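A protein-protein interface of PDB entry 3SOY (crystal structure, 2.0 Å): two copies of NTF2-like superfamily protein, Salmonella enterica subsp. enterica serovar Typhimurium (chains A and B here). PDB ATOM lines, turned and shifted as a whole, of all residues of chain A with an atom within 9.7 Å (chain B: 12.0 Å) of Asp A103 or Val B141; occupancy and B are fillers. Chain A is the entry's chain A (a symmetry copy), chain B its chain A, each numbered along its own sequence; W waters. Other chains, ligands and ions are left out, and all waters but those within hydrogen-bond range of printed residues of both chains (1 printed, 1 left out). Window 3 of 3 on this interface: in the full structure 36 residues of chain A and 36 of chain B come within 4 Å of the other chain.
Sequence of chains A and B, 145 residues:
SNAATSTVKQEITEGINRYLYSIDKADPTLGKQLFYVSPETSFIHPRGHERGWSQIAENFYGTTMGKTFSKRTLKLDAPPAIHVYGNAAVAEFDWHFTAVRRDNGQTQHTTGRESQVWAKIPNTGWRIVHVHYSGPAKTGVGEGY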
ATOM      1  N   ARG A  47     -32.772  -5.313 -11.391  1.00  0.00           N
ATOM      2  CA  ARG A  47     -32.010  -6.554 -11.257  1.00  0.00           C
ATOM      3  C   ARG A  47     -32.772  -7.840 -11.556  1.00  0.00           C
ATOM      4  O   ARG A  47     -32.196  -8.962 -11.542  1.00  0.00           O
ATOM      5  CB  ARG A  47     -31.402  -6.622  -9.857  1.00  0.00           C
ATOM      6  CG  ARG A  47     -30.291  -5.619  -9.655  1.00  0.00           C
ATOM      7  CD  ARG A  47     -29.711  -5.678  -8.232  1.00  0.00           C
ATOM      8  NE  ARG A  47     -28.942  -6.887  -7.981  1.00  0.00           N
ATOM      9  CZ  ARG A  47     -27.702  -7.109  -8.395  1.00  0.00           C
ATOM     10  NH1 ARG A  47     -27.042  -6.218  -9.131  1.00  0.00           N
ATOM     11  NH2 ARG A  47     -27.138  -8.259  -8.110  1.00  0.00           N
ATOM     12  N   GLY A  66     -31.982  -6.646   2.079  1.00  0.00           N
ATOM     13  CA  GLY A  66     -31.479  -7.047   3.406  1.00  0.00           C
ATOM     14  C   GLY A  66     -30.093  -7.668   3.489  1.00  0.00           C
ATOM     15  O   GLY A  66     -29.364  -7.424   4.443  1.00  0.00           O
ATOM     16  N   LYS A  67     -29.705  -8.480   2.514  1.00  0.00           N
ATOM     17  CA  LYS A  67     -28.352  -9.018   2.522  1.00  0.00           C
ATOM     18  C   LYS A  67     -27.336  -8.067   1.871  1.00  0.00           C
ATOM     19  O   LYS A  67     -26.147  -8.079   2.205  1.00  0.00           O
ATOM     20  CB  LYS A  67     -28.295 -10.381   1.842  1.00  0.00           C
ATOM     21  CG  LYS A  67     -29.029 -11.486   2.580  1.00  0.00           C
ATOM     22  CD  LYS A  67     -29.096 -12.798   1.729  1.00  0.00           C
ATOM     23  CE  LYS A  67     -29.456 -14.030   2.624  1.00  0.00           C
ATOM     24  NZ  LYS A  67     -30.788 -13.829   3.312  1.00  0.00           N
ATOM     25  N   THR A  68     -27.798  -7.233   0.960  1.00  0.00           N
ATOM     26  CA  THR A  68     -26.888  -6.399   0.194  1.00  0.00           C
ATOM     27  C   THR A  68     -26.440  -5.173   0.997  1.00  0.00           C
ATOM     28  O   THR A  68     -25.297  -4.748   0.874  1.00  0.00           O
ATOM     29  CB  THR A  68     -27.531  -6.026  -1.151  1.00  0.00           C
ATOM     30  OG1 THR A  68     -27.802  -7.237  -1.875  1.00  0.00           O
ATOM     31  CG2 THR A  68     -26.602  -5.140  -1.984  1.00  0.00           C
ATOM     32  N   PHE A  69     -27.330  -4.633   1.845  1.00  0.00           N
ATOM     33  CA  PHE A  69     -27.102  -3.354   2.538  1.00  0.00           C
ATOM     34  C   PHE A  69     -27.289  -3.498   4.036  1.00  0.00           C
ATOM     35  O   PHE A  69     -28.137  -4.274   4.471  1.00  0.00           O
ATOM     36  CB  PHE A  69     -28.075  -2.283   2.032  1.00  0.00           C
ATOM     37  CG  PHE A  69     -27.993  -2.036   0.547  1.00  0.00           C
ATOM     38  CD1 PHE A  69     -26.892  -1.365   0.007  1.00  0.00           C
ATOM     39  CD2 PHE A  69     -28.999  -2.506  -0.317  1.00  0.00           C
ATOM     40  CE1 PHE A  69     -26.779  -1.154  -1.374  1.00  0.00           C
ATOM     41  CE2 PHE A  69     -28.909  -2.304  -1.695  1.00  0.00           C
ATOM     42  CZ  PHE A  69     -27.799  -1.619  -2.237  1.00  0.00           C
ATOM     43  N   SER A  70     -26.524  -2.742   4.815  1.00  0.00           N
ATOM     44  CA  SER A  70     -26.649  -2.781   6.257  1.00  0.00           C
ATOM     45  C   SER A  70     -27.506  -1.622   6.762  1.00  0.00           C
ATOM     46  O   SER A  70     -28.002  -1.664   7.878  1.00  0.00           O
ATOM     47  CB  SER A  70     -25.279  -2.748   6.916  1.00  0.00           C
ATOM     48  OG  SER A  70     -24.542  -1.629   6.496  1.00  0.00           O
ATOM     49  N   LYS A  71     -27.622  -0.558   5.979  1.00  0.00           N
ATOM     50  CA  LYS A  71     -28.498   0.574   6.335  1.00  0.00           C
ATOM     51  C   LYS A  71     -29.131   1.046   5.011  1.00  0.00           C
ATOM     52  O   LYS A  71     -28.483   0.982   3.966  1.00  0.00           O
ATOM     53  CB  LYS A  71     -27.750   1.702   7.075  1.00  0.00           C
ATOM     54  N   ALA A  99     -28.000   3.760   0.754  1.00  0.00           N
ATOM     55  CA  ALA A  99     -27.777   2.528   1.431  1.00  0.00           C
ATOM     56  C   ALA A  99     -26.285   2.367   1.675  1.00  0.00           C
ATOM     57  O   ALA A  99     -25.465   2.838   0.867  1.00  0.00           O
ATOM     58  CB  ALA A  99     -28.360   1.370   0.613  1.00  0.00           C
ATOM     59  N   VAL A 100     -25.943   1.738   2.800  1.00  0.00           N
ATOM     60  CA  VAL A 100     -24.603   1.278   3.052  1.00  0.00           C
ATOM     61  C   VAL A 100     -24.536  -0.210   2.621  1.00  0.00           C
ATOM     62  O   VAL A 100     -25.289  -1.053   3.129  1.00  0.00           O
ATOM     63  CB  VAL A 100     -24.206   1.470   4.556  1.00  0.00           C
ATOM     64  CG1 VAL A 100     -22.715   1.138   4.780  1.00  0.00           C
ATOM     65  CG2 VAL A 100     -24.564   2.901   5.046  1.00  0.00           C
ATOM     66  N   ARG A 101     -23.620  -0.522   1.696  1.00  0.00           N
ATOM     67  CA  ARG A 101     -23.321  -1.910   1.309  1.00  0.00           C
ATOM     68  C   ARG A 101     -22.614  -2.784   2.379  1.00  0.00           C
ATOM     69  O   ARG A 101     -21.642  -2.355   3.009  1.00  0.00           O
ATOM     70  CB  ARG A 101     -22.369  -1.936   0.127  1.00  0.00           C
ATOM     71  CG  ARG A 101     -22.792  -1.255  -1.115  1.00  0.00           C
ATOM     72  CD  ARG A 101     -22.018  -1.912  -2.256  1.00  0.00           C
ATOM     73  NE  ARG A 101     -21.628  -0.948  -3.278  1.00  0.00           N
ATOM     74  CZ  ARG A 101     -20.826  -1.203  -4.319  1.00  0.00           C
ATOM     75  NH1 ARG A 101     -20.296  -2.423  -4.513  1.00  0.00           N
ATOM     76  NH2 ARG A 101     -20.558  -0.223  -5.181  1.00  0.00           N
ATOM     77  N   ARG A 102     -23.061  -4.033   2.521  1.00  0.00           N
ATOM     78  CA  ARG A 102     -22.357  -5.015   3.356  1.00  0.00           C
ATOM     79  C   ARG A 102     -20.999  -5.446   2.782  1.00  0.00           C
ATOM     80  O   ARG A 102     -20.098  -5.742   3.547  1.00  0.00           O
ATOM     81  CB  ARG A 102     -23.190  -6.270   3.559  1.00  0.00           C
ATOM     82  CG  ARG A 102     -24.388  -6.052   4.410  1.00  0.00           C
ATOM     83  CD  ARG A 102     -24.910  -7.372   4.969  1.00  0.00           C
ATOM     84  NE  ARG A 102     -26.313  -7.213   5.343  1.00  0.00           N
ATOM     85  CZ  ARG A 102     -26.742  -6.834   6.543  1.00  0.00           C
ATOM     86  NH1 ARG A 102     -28.041  -6.691   6.738  1.00  0.00           N
ATOM     87  NH2 ARG A 102     -25.886  -6.603   7.546  1.00  0.00           N
ATOM     88  N   ASP A 103     -20.864  -5.510   1.452  1.00  0.00           N
ATOM     89  CA  ASP A 103     -19.633  -6.076   0.841  1.00  0.00           C
ATOM     90  C   ASP A 103     -18.389  -5.199   1.118  1.00  0.00           C
ATOM     91  O   ASP A 103     -17.369  -5.728   1.548  1.00  0.00           O
ATOM     92  CB  ASP A 103     -19.795  -6.481  -0.667  1.00  0.00           C
ATOM     93  CG  ASP A 103     -20.290  -5.338  -1.587  1.00  0.00           C
ATOM     94  OD1 ASP A 103     -20.044  -4.163  -1.267  1.00  0.00           O
ATOM     95  OD2 ASP A 103     -20.923  -5.625  -2.659  1.00  0.00           O
ATOM     96  N   ASN A 104     -18.504  -3.875   0.945  1.00  0.00           N
ATOM     97  CA  ASN A 104     -17.363  -2.950   1.096  1.00  0.00           C
ATOM     98  C   ASN A 104     -17.560  -1.776   2.077  1.00  0.00           C
ATOM     99  O   ASN A 104     -16.686  -0.916   2.210  1.00  0.00           O
ATOM    100  CB  ASN A 104     -16.973  -2.404  -0.285  1.00  0.00           C
ATOM    101  CG  ASN A 104     -18.052  -1.516  -0.900  1.00  0.00           C
ATOM    102  OD1 ASN A 104     -19.030  -1.164  -0.246  1.00  0.00           O
ATOM    103  ND2 ASN A 104     -17.872  -1.151  -2.174  1.00  0.00           N
ATOM    104  N   GLY A 105     -18.716  -1.729   2.736  1.00  0.00           N
ATOM    105  CA  GLY A 105     -19.037  -0.654   3.698  1.00  0.00           C
ATOM    106  C   GLY A 105     -19.372   0.717   3.109  1.00  0.00           C
ATOM    107  O   GLY A 105     -19.751   1.643   3.825  1.00  0.00           O
ATOM    108  N   GLN A 106     -19.254   0.853   1.798  1.00  0.00           N
ATOM    109  CA  GLN A 106     -19.453   2.143   1.170  1.00  0.00           C
ATOM    110  C   GLN A 106     -20.926   2.505   1.003  1.00  0.00           C
ATOM    111  O   GLN A 106     -21.754   1.629   0.780  1.00  0.00           O
ATOM    112  CB  GLN A 106     -18.742   2.166  -0.162  1.00  0.00           C
ATOM    113  CG  GLN A 106     -17.245   2.277   0.009  1.00  0.00           C
ATOM    114  CD  GLN A 106     -16.549   2.258  -1.331  1.00  0.00           C
ATOM    115  OE1 GLN A 106     -17.202   2.139  -2.383  1.00  0.00           O
ATOM    116  NE2 GLN A 106     -15.219   2.374  -1.313  1.00  0.00           N
ATOM    117  N   THR A 107     -21.221   3.801   1.151  1.00  0.00           N
ATOM    118  CA  THR A 107     -22.557   4.369   0.917  1.00  0.00           C
ATOM    119  C   THR A 107     -22.835   4.539  -0.578  1.00  0.00           C
ATOM    120  O   THR A 107     -22.078   5.201  -1.280  1.00  0.00           O
ATOM    121  CB  THR A 107     -22.744   5.750   1.573  1.00  0.00           C
ATOM    122  OG1 THR A 107     -22.708   5.618   2.993  1.00  0.00           O
ATOM    123  CG2 THR A 107     -24.084   6.349   1.174  1.00  0.00           C
ATOM    124  N   GLN A 108     -23.936   3.945  -1.039  1.00  0.00           N
ATOM    125  CA  GLN A 108     -24.317   3.945  -2.439  1.00  0.00           C
ATOM    126  C   GLN A 108     -25.613   4.781  -2.533  1.00  0.00           C
ATOM    127  O   GLN A 108     -26.488   4.752  -1.625  1.00  0.00           O
ATOM    128  CB  GLN A 108     -24.422   2.479  -2.906  1.00  0.00           C
ATOM    129  CG  GLN A 108     -25.196   2.176  -4.154  1.00  0.00           C
ATOM    130  CD  GLN A 108     -24.863   0.767  -4.796  1.00  0.00           C
ATOM    131  OE1 GLN A 108     -24.595  -0.270  -4.116  1.00  0.00           O
ATOM    132  NE2 GLN A 108     -24.896   0.752  -6.130  1.00  0.00           N
ATOM    133  N   ALA B 137     -32.787  -6.705 -17.271  1.00  0.00           N
ATOM    134  CA  ALA B 137     -32.215  -6.837 -15.950  1.00  0.00           C
ATOM    135  C   ALA B 137     -30.697  -6.798 -16.071  1.00  0.00           C
ATOM    136  O   ALA B 137     -30.137  -7.236 -17.082  1.00  0.00           O
ATOM    137  CB  ALA B 137     -32.688  -8.131 -15.263  1.00  0.00           C
ATOM    138  N   LYS B 138     -30.065  -6.182 -15.073  1.00  0.00           N
ATOM    139  CA  LYS B 138     -28.594  -6.126 -14.939  1.00  0.00           C
ATOM    140  C   LYS B 138     -28.272  -6.660 -13.583  1.00  0.00           C
ATOM    141  O   LYS B 138     -28.821  -6.153 -12.597  1.00  0.00           O
ATOM    142  CB  LYS B 138     -28.084  -4.693 -14.948  1.00  0.00           C
ATOM    143  CG  LYS B 138     -28.251  -3.924 -16.260  1.00  0.00           C
ATOM    144  CD  LYS B 138     -27.874  -2.417 -16.031  1.00  0.00           C
ATOM    145  CE  LYS B 138     -28.709  -1.810 -14.862  1.00  0.00           C
ATOM    146  NZ  LYS B 138     -29.141  -0.404 -15.102  1.00  0.00           N
ATOM    147  N   THR B 139     -27.393  -7.656 -13.522  1.00  0.00           N
ATOM    148  CA  THR B 139     -27.139  -8.351 -12.272  1.00  0.00           C
ATOM    149  C   THR B 139     -25.675  -8.200 -11.816  1.00  0.00           C
ATOM    150  O   THR B 139     -25.215  -8.940 -10.976  1.00  0.00           O
ATOM    151  CB  THR B 139     -27.662  -9.889 -12.310  1.00  0.00           C
ATOM    152  OG1 THR B 139     -26.819 -10.734 -13.116  1.00  0.00           O
ATOM    153  CG2 THR B 139     -29.165 -10.048 -12.809  1.00  0.00           C
ATOM    154  N   GLY B 140     -24.939  -7.235 -12.355  1.00  0.00           N
ATOM    155  CA  GLY B 140     -23.542  -7.055 -11.964  1.00  0.00           C
ATOM    156  C   GLY B 140     -23.449  -6.579 -10.527  1.00  0.00           C
ATOM    157  O   GLY B 140     -24.457  -6.185  -9.968  1.00  0.00           O
ATOM    158  N   VAL B 141     -22.252  -6.617  -9.926  1.00  0.00           N
ATOM    159  CA  VAL B 141     -22.059  -6.138  -8.558  1.00  0.00           C
ATOM    160  C   VAL B 141     -22.243  -4.622  -8.565  1.00  0.00           C
ATOM    161  O   VAL B 141     -21.683  -3.906  -9.410  1.00  0.00           O
ATOM    162  CB  VAL B 141     -20.662  -6.511  -7.965  1.00  0.00           C
ATOM    163  CG1 VAL B 141     -20.513  -5.953  -6.547  1.00  0.00           C
ATOM    164  CG2 VAL B 141     -20.444  -8.046  -7.967  1.00  0.00           C
ATOM    165  N   GLY B 142     -23.085  -4.147  -7.645  1.00  0.00           N
ATOM    166  CA  GLY B 142     -23.341  -2.731  -7.491  1.00  0.00           C
ATOM    167  C   GLY B 142     -24.317  -2.126  -8.493  1.00  0.00           C
ATOM    168  O   GLY B 142     -24.630  -0.947  -8.387  1.00  0.00           O
ATOM    169  N   GLU B 143     -24.823  -2.871  -9.470  1.00  0.00           N
ATOM    170  CA  GLU B 143     -25.703  -2.210 -10.458  1.00  0.00           C
ATOM    171  C   GLU B 143     -27.175  -2.544 -10.263  1.00  0.00           C
ATOM    172  O   GLU B 143     -27.518  -3.574  -9.711  1.00  0.00           O
ATOM    173  CB  GLU B 143     -25.282  -2.448 -11.916  1.00  0.00           C
ATOM    174  CG  GLU B 143     -24.617  -3.767 -12.263  1.00  0.00           C
ATOM    175  CD  GLU B 143     -24.560  -4.025 -13.817  1.00  0.00           C
ATOM    176  OE1 GLU B 143     -24.598  -5.208 -14.271  1.00  0.00           O
ATOM    177  OE2 GLU B 143     -24.510  -3.032 -14.583  1.00  0.00           O
ATOM    178  N   GLY B 144     -28.029  -1.657 -10.752  1.00  0.00           N
ATOM    179  CA  GLY B 144     -29.475  -1.867 -10.771  1.00  0.00           C
ATOM    180  C   GLY B 144     -30.246  -1.566  -9.479  1.00  0.00           C
ATOM    181  O   GLY B 144     -31.392  -2.006  -9.319  1.00  0.00           O
ATOM    182  N   TYR B 145     -29.660  -0.783  -8.584  1.00  0.00           N
ATOM    183  CA  TYR B 145     -30.364  -0.373  -7.364  1.00  0.00           C
ATOM    184  C   TYR B 145     -30.906   1.081  -7.539  1.00  0.00           C
ATOM    185  O   TYR B 145     -30.803   1.603  -8.663  1.00  0.00           O
ATOM    186  CB  TYR B 145     -29.437  -0.501  -6.152  1.00  0.00           C
ATOM    187  CG  TYR B 145     -28.830  -1.881  -5.964  1.00  0.00           C
ATOM    188  CD1 TYR B 145     -29.512  -2.877  -5.273  1.00  0.00           C
ATOM    189  CD2 TYR B 145     -27.562  -2.177  -6.441  1.00  0.00           C
ATOM    190  CE1 TYR B 145     -28.962  -4.140  -5.079  1.00  0.00           C
ATOM    191  CE2 TYR B 145     -27.000  -3.450  -6.271  1.00  0.00           C
ATOM    192  CZ  TYR B 145     -27.712  -4.427  -5.590  1.00  0.00           C
ATOM    193  OH  TYR B 145     -27.177  -5.696  -5.433  1.00  0.00           O
ATOM    194  OXT TYR B 145     -31.460   1.789  -6.631  1.00  0.00           O
HETATM  195  O   HOH W   1     -28.302  -8.199  -4.587  1.00  0.00           O
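The backbone carbonyl oxygen (O) of Gly B140 sits at hydrogen-bond distance from the guanidinium group (NH1) of Arg A47.
O of Gly B142 is in hydrogen-bond range of NE2 of Gln A108, at 2.8 Å.
O of Glu B143 lies within hydrogen-bond range of NH1 of Arg A47 (2.7 Å).
NE of Arg A47 is in hydrogen-bond range of OH of Tyr B145.
The backbone NH (N) of Gly B140 sits at hydrogen-bond distance from the side-chain carboxylate (OE1) of Glu B143 (2.8 Å).
The backbone carbonyl oxygen of Phe A69 is in hydrogen-bond range of the guanidinium group of Arg A102, 3.3 Å away.
The backbone NH (N) of Gln A108 is in hydrogen-bond range of the backbone carbonyl oxygen (O) of Ala A99 (2.7 Å).
The guanidinium group (NH1) of Arg A101 lies within salt-bridge range of the side-chain carboxylate (OD1) of Asp A103.
NE of Arg A101 lies within hydrogen-bond range of OE1 of Gln A108 (3.2 Å).
The side-chain carboxylate (OD1) of Asp A103 lies close to the side-chain amide oxygen (OD1) of Asn A104 (3.3 Å).
Ala B137 touches Arg A47.
Arg A47 touches Lys B138.
Arg A47 touches Thr B139.
Arg A47 touches Gly B144 (CG to O, 3.8 Å).
Tyr B145 touches Thr A68 (OH to CG2, 3.5 Å).
Phe A69 touches Tyr B145 (CE2 to CD1, 3.7 Å).
OD2 of Asp A103 touches CG1 of Val B141, 3.9 Å away.
Gln A108 touches Tyr B145.
Of the printed residues of chain B, Arg A47 touches Ala B137, Lys B138, Thr B139, Gly B140, Glu B143, Gly B144 and Tyr B145.
Of chain B, only Tyr B145 (3.5 Å) comes within 4 Å of Thr A68.
Lys A71 touches none of the printed residues of chain B.
Arg A101 touches none of the printed residues of chain B.
Asp A103 touches just one residue of chain B: Val B141.
Asn A104 touches none of the printed residues of chain B.
No residue of chain B comes within 4 Å of Gly A105.
Printed residues of chain B within 4 Å of Gln A108: Gly B142 (2.8 Å) and Tyr B145 (3.97 Å).
Printed residues of chain A within 4 Å of Ala B137: Arg A47.
Printed residues of chain A within 4 Å of Lys B138: Arg A47 (3.3 Å).
Of chain A, only Arg A47 comes within 4 Å of Gly B140.
Val B141 touches just one residue of chain A: Asp A103 (3.9 Å).
Gly B142 touches just one residue of chain A: Gln A108 (2.8 Å).
Of the printed residues of chain A, Tyr B145 touches Arg A47 (3.3 Å), Thr A68 (3.5 Å), Phe A69 (3.7 Å) and Gln A108 (3.97 Å).
The nearest residue of chain B that does not touch Asp A103 is Gly B142 (5.6 Å).
The nearest printed residue of chain B that does not touch Phe A69 is Gly B142 (7.0 Å).
Printed residues of chain B that touch a printed residue of chain A: Ala B137, Lys B138, Thr B139, Gly B140, Val B141, Gly B142, Glu B143, Gly B144 and Tyr B145.
Hydrophobic or aromatic side chains of chain B within 4 Å of the printed part of chain A: Ala B137, Val B141 and Tyr B145.
Along chain B the printed residues that touch a printed residue of chain A span positions 137 to 145.
Of the 17 printed residues of chain A, 5 touch a printed residue of chain B.
Printed residues of chain A that touch a printed residue of chain B: Arg A47, Thr A68, Phe A69, Asp A103 and Gln A108.
Hydrophobic or aromatic side chains of chain A within 4 Å of the printed part of chain B: Phe A69.
No position is printed for both chains.
Of the 12 pairs that touch across the chains among the printed residues, none has its exchanged pair printed and touching as well.
Water W1 bridges OH of Tyr B145 (2.9 Å) and OG1 of Thr A68 (2.9 Å).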
